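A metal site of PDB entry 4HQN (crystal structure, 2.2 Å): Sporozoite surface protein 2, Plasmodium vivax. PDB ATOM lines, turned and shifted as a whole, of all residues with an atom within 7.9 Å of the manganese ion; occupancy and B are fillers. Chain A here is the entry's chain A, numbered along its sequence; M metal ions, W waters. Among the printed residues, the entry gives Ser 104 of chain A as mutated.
N of Ser 28 sits at hydrogen-bond distance from OD1 of Asp 26. N of Val 136 sits at hydrogen-bond distance from OD1 of Asp 134, 3.2 Å away. OG of Ser 30 sits close to OD2 of Asp 134, at 2.5 Å. The backbone NH (N) of Thr 103 lies within hydrogen-bond range of the side-chain amide oxygen (OD1) of Asn 138 (2.8 Å).
Merely in contact with the manganese ion: Val 136. Within 4 Å of the manganese ion: Ser 28, Ser 30, Thr 103 and Val 136.
The manganese ion is bound by water W3 (2.1 Å), OG of Ser 30 (2.1 Å), water W2 (2.2 Å), water W1 (2.2 Å), OG1 of Thr 103 (2.2 Å) and OG of Ser 28 (2.2 Å).
Water W3 lies within hydrogen-bond range of N of Ser 30 (3.0 Å) and O of Gly 101 (3.1 Å).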
ATOM      1  N   ASP A  26      -2.822 -18.721 -18.554  1.00  0.00           N
ATOM      2  CA  ASP A  26      -1.973 -18.320 -17.430  1.00  0.00           C
ATOM      3  C   ASP A  26      -0.673 -17.722 -17.947  1.00  0.00           C
ATOM      4  O   ASP A  26       0.138 -18.436 -18.540  1.00  0.00           O
ATOM      5  CB  ASP A  26      -1.657 -19.558 -16.575  1.00  0.00           C
ATOM      6  CG  ASP A  26      -1.032 -19.211 -15.227  1.00  0.00           C
ATOM      7  OD1 ASP A  26      -0.323 -18.188 -15.128  1.00  0.00           O
ATOM      8  OD2 ASP A  26      -1.271 -19.983 -14.258  1.00  0.00           O
ATOM      9  N   GLY A  27      -0.441 -16.430 -17.735  1.00  0.00           N
ATOM     10  CA  GLY A  27       0.805 -15.809 -18.140  1.00  0.00           C
ATOM     11  C   GLY A  27       1.707 -15.395 -16.978  1.00  0.00           C
ATOM     12  O   GLY A  27       2.537 -14.489 -17.120  1.00  0.00           O
ATOM     13  N   SER A  28       1.571 -16.069 -15.837  1.00  0.00           N
ATOM     14  CA  SER A  28       2.233 -15.644 -14.608  1.00  0.00           C
ATOM     15  C   SER A  28       3.655 -16.193 -14.465  1.00  0.00           C
ATOM     16  O   SER A  28       4.038 -17.126 -15.180  1.00  0.00           O
ATOM     17  CB  SER A  28       1.404 -16.070 -13.384  1.00  0.00           C
ATOM     18  OG  SER A  28       1.388 -17.471 -13.247  1.00  0.00           O
ATOM     19  N   GLY A  29       4.410 -15.632 -13.532  1.00  0.00           N
ATOM     20  CA  GLY A  29       5.812 -16.003 -13.358  1.00  0.00           C
ATOM     21  C   GLY A  29       6.038 -17.453 -13.013  1.00  0.00           C
ATOM     22  O   GLY A  29       7.108 -17.994 -13.283  1.00  0.00           O
ATOM     23  N   SER A  30       5.056 -18.116 -12.417  1.00  0.00           N
ATOM     24  CA  SER A  30       5.216 -19.529 -12.093  1.00  0.00           C
ATOM     25  C   SER A  30       5.338 -20.429 -13.342  1.00  0.00           C
ATOM     26  O   SER A  30       5.882 -21.526 -13.270  1.00  0.00           O
ATOM     27  CB  SER A  30       4.101 -20.048 -11.148  1.00  0.00           C
ATOM     28  OG  SER A  30       2.822 -19.969 -11.727  1.00  0.00           O
ATOM     29  N   ILE A  31       4.824 -19.972 -14.475  1.00  0.00           N
ATOM     30  CA  ILE A  31       4.836 -20.825 -15.681  1.00  0.00           C
ATOM     31  C   ILE A  31       6.260 -21.232 -16.089  1.00  0.00           C
ATOM     32  O   ILE A  31       6.531 -22.420 -16.325  1.00  0.00           O
ATOM     33  CB  ILE A  31       4.101 -20.154 -16.855  1.00  0.00           C
ATOM     34  CG1 ILE A  31       2.624 -19.946 -16.517  1.00  0.00           C
ATOM     35  CG2 ILE A  31       4.280 -20.962 -18.150  1.00  0.00           C
ATOM     36  CD1 ILE A  31       1.875 -21.247 -16.115  1.00  0.00           C
ATOM     37  N   GLY A  32       7.176 -20.274 -16.140  1.00  0.00           N
ATOM     38  CA  GLY A  32       8.567 -20.537 -16.478  1.00  0.00           C
ATOM     39  C   GLY A  32       8.834 -20.199 -17.940  1.00  0.00           C
ATOM     40  O   GLY A  32       8.106 -20.649 -18.833  1.00  0.00           O
ATOM     41  N   PHE A  65      -3.749 -13.958 -18.217  1.00  0.00           N
ATOM     42  CA  PHE A  65      -3.788 -13.529 -16.835  1.00  0.00           C
ATOM     43  C   PHE A  65      -2.493 -13.757 -16.086  1.00  0.00           C
ATOM     44  O   PHE A  65      -1.919 -14.850 -16.100  1.00  0.00           O
ATOM     45  CB  PHE A  65      -5.000 -14.102 -16.074  1.00  0.00           C
ATOM     46  CG  PHE A  65      -4.983 -15.596 -15.908  1.00  0.00           C
ATOM     47  CD1 PHE A  65      -5.567 -16.417 -16.866  1.00  0.00           C
ATOM     48  CD2 PHE A  65      -4.405 -16.181 -14.791  1.00  0.00           C
ATOM     49  CE1 PHE A  65      -5.575 -17.814 -16.719  1.00  0.00           C
ATOM     50  CE2 PHE A  65      -4.419 -17.568 -14.624  1.00  0.00           C
ATOM     51  CZ  PHE A  65      -4.993 -18.386 -15.591  1.00  0.00           C
ATOM     52  N   GLY A  66      -2.023 -12.679 -15.467  1.00  0.00           N
ATOM     53  CA  GLY A  66      -0.827 -12.680 -14.641  1.00  0.00           C
ATOM     54  C   GLY A  66      -1.159 -11.810 -13.440  1.00  0.00           C
ATOM     55  O   GLY A  66      -2.184 -12.022 -12.798  1.00  0.00           O
ATOM     56  N   TYR A 100       5.394 -13.347 -16.055  1.00  0.00           N
ATOM     57  CA  TYR A 100       5.896 -12.758 -14.835  1.00  0.00           C
ATOM     58  C   TYR A 100       4.711 -12.521 -13.901  1.00  0.00           C
ATOM     59  O   TYR A 100       3.552 -12.521 -14.329  1.00  0.00           O
ATOM     60  CB  TYR A 100       6.600 -11.432 -15.134  1.00  0.00           C
ATOM     61  CG  TYR A 100       5.606 -10.313 -15.302  1.00  0.00           C
ATOM     62  CD1 TYR A 100       4.883 -10.187 -16.491  1.00  0.00           C
ATOM     63  CD2 TYR A 100       5.356  -9.406 -14.263  1.00  0.00           C
ATOM     64  CE1 TYR A 100       3.933  -9.180 -16.658  1.00  0.00           C
ATOM     65  CE2 TYR A 100       4.398  -8.411 -14.420  1.00  0.00           C
ATOM     66  CZ  TYR A 100       3.693  -8.301 -15.616  1.00  0.00           C
ATOM     67  OH  TYR A 100       2.753  -7.299 -15.761  1.00  0.00           O
ATOM     68  N   GLY A 101       4.994 -12.301 -12.627  1.00  0.00           N
ATOM     69  CA  GLY A 101       3.989 -11.802 -11.709  1.00  0.00           C
ATOM     70  C   GLY A 101       3.098 -12.868 -11.083  1.00  0.00           C
ATOM     71  O   GLY A 101       3.382 -14.065 -11.135  1.00  0.00           O
ATOM     72  N   THR A 102       2.007 -12.401 -10.499  1.00  0.00           N
ATOM     73  CA  THR A 102       1.110 -13.266  -9.772  1.00  0.00           C
ATOM     74  C   THR A 102       0.066 -13.824 -10.746  1.00  0.00           C
ATOM     75  O   THR A 102       0.252 -13.741 -11.967  1.00  0.00           O
ATOM     76  CB  THR A 102       0.487 -12.548  -8.536  1.00  0.00           C
ATOM     77  OG1 THR A 102      -0.041 -11.281  -8.916  1.00  0.00           O
ATOM     78  CG2 THR A 102       1.566 -12.310  -7.452  1.00  0.00           C
ATOM     79  N   THR A 103      -1.013 -14.403 -10.238  1.00  0.00           N
ATOM     80  CA  THR A 103      -1.833 -15.278 -11.046  1.00  0.00           C
ATOM     81  C   THR A 103      -3.328 -14.982 -10.846  1.00  0.00           C
ATOM     82  O   THR A 103      -3.992 -15.642 -10.034  1.00  0.00           O
ATOM     83  CB  THR A 103      -1.532 -16.753 -10.700  1.00  0.00           C
ATOM     84  OG1 THR A 103      -0.112 -16.945 -10.632  1.00  0.00           O
ATOM     85  CG2 THR A 103      -2.149 -17.712 -11.738  1.00  0.00           C
ATOM     86  N   SER A 104      -3.834 -13.988 -11.576  1.00  0.00           N
ATOM     87  CA  SER A 104      -5.227 -13.519 -11.440  1.00  0.00           C
ATOM     88  C   SER A 104      -6.255 -14.446 -12.063  1.00  0.00           C
ATOM     89  O   SER A 104      -7.026 -14.028 -12.927  1.00  0.00           O
ATOM     90  CB  SER A 104      -5.394 -12.165 -12.126  1.00  0.00           C
ATOM     91  OG  SER A 104      -4.830 -11.124 -11.362  1.00  0.00           O
ATOM     92  N   MET A 105      -6.263 -15.695 -11.607  1.00  0.00           N
ATOM     93  CA  MET A 105      -7.148 -16.692 -12.197  1.00  0.00           C
ATOM     94  C   MET A 105      -8.623 -16.383 -11.944  1.00  0.00           C
ATOM     95  O   MET A 105      -9.446 -16.505 -12.844  1.00  0.00           O
ATOM     96  CB  MET A 105      -6.801 -18.091 -11.685  1.00  0.00           C
ATOM     97  CG  MET A 105      -7.593 -19.189 -12.358  1.00  0.00           C
ATOM     98  SD  MET A 105      -7.305 -20.814 -11.613  1.00  0.00           S
ATOM     99  CE  MET A 105      -5.594 -21.029 -12.059  1.00  0.00           C
ATOM    100  N   THR A 133      -3.511 -23.425 -17.324  1.00  0.00           N
ATOM    101  CA  THR A 133      -2.853 -22.959 -16.098  1.00  0.00           C
ATOM    102  C   THR A 133      -1.986 -24.047 -15.444  1.00  0.00           C
ATOM    103  O   THR A 133      -2.138 -25.233 -15.760  1.00  0.00           O
ATOM    104  CB  THR A 133      -3.877 -22.446 -15.072  1.00  0.00           C
ATOM    105  OG1 THR A 133      -3.202 -22.072 -13.869  1.00  0.00           O
ATOM    106  CG2 THR A 133      -4.886 -23.508 -14.726  1.00  0.00           C
ATOM    107  N   ASP A 134      -1.050 -23.649 -14.580  1.00  0.00           N
ATOM    108  CA  ASP A 134      -0.346 -24.632 -13.732  1.00  0.00           C
ATOM    109  C   ASP A 134      -1.146 -24.956 -12.467  1.00  0.00           C
ATOM    110  O   ASP A 134      -0.768 -25.833 -11.679  1.00  0.00           O
ATOM    111  CB  ASP A 134       1.077 -24.182 -13.376  1.00  0.00           C
ATOM    112  CG  ASP A 134       1.116 -22.887 -12.586  1.00  0.00           C
ATOM    113  OD1 ASP A 134       0.049 -22.365 -12.193  1.00  0.00           O
ATOM    114  OD2 ASP A 134       2.222 -22.357 -12.370  1.00  0.00           O
ATOM    115  N   GLY A 135      -2.237 -24.227 -12.278  1.00  0.00           N
ATOM    116  CA  GLY A 135      -3.174 -24.548 -11.215  1.00  0.00           C
ATOM    117  C   GLY A 135      -2.721 -24.041  -9.868  1.00  0.00           C
ATOM    118  O   GLY A 135      -2.995 -24.660  -8.840  1.00  0.00           O
ATOM    119  N   VAL A 136      -2.029 -22.916  -9.867  1.00  0.00           N
ATOM    120  CA  VAL A 136      -1.555 -22.284  -8.643  1.00  0.00           C
ATOM    121  C   VAL A 136      -1.989 -20.842  -8.684  1.00  0.00           C
ATOM    122  O   VAL A 136      -1.217 -19.953  -9.005  1.00  0.00           O
ATOM    123  CB  VAL A 136      -0.023 -22.363  -8.523  1.00  0.00           C
ATOM    124  CG1 VAL A 136       0.453 -21.680  -7.221  1.00  0.00           C
ATOM    125  CG2 VAL A 136       0.411 -23.820  -8.522  1.00  0.00           C
ATOM    126  N   PRO A 137      -3.261 -20.599  -8.369  1.00  0.00           N
ATOM    127  CA  PRO A 137      -3.824 -19.260  -8.525  1.00  0.00           C
ATOM    128  C   PRO A 137      -3.505 -18.398  -7.313  1.00  0.00           C
ATOM    129  O   PRO A 137      -2.999 -18.926  -6.319  1.00  0.00           O
ATOM    130  CB  PRO A 137      -5.315 -19.547  -8.593  1.00  0.00           C
ATOM    131  CG  PRO A 137      -5.486 -20.742  -7.699  1.00  0.00           C
ATOM    132  CD  PRO A 137      -4.263 -21.575  -7.925  1.00  0.00           C
ATOM    133  N   ASN A 138      -3.779 -17.103  -7.395  1.00  0.00           N
ATOM    134  CA  ASN A 138      -3.640 -16.230  -6.249  1.00  0.00           C
ATOM    135  C   ASN A 138      -4.390 -16.753  -5.010  1.00  0.00           C
ATOM    136  O   ASN A 138      -3.876 -16.654  -3.900  1.00  0.00           O
ATOM    137  CB  ASN A 138      -4.102 -14.816  -6.586  1.00  0.00           C
ATOM    138  CG  ASN A 138      -3.103 -14.077  -7.466  1.00  0.00           C
ATOM    139  OD1 ASN A 138      -1.958 -14.506  -7.649  1.00  0.00           O
ATOM    140  ND2 ASN A 138      -3.527 -12.923  -7.978  1.00  0.00           N
HETATM  141 MN    MN M   1       1.358 -18.464 -11.269  1.00  0.00          MN
HETATM  142  O   HOH W   1       0.014 -20.029 -12.022  1.00  0.00           O
HETATM  143  O   HOH W   2       1.246 -19.183  -9.234  1.00  0.00           O
HETATM  144  O   HOH W   3       2.841 -17.042 -10.653  1.00  0.00           O
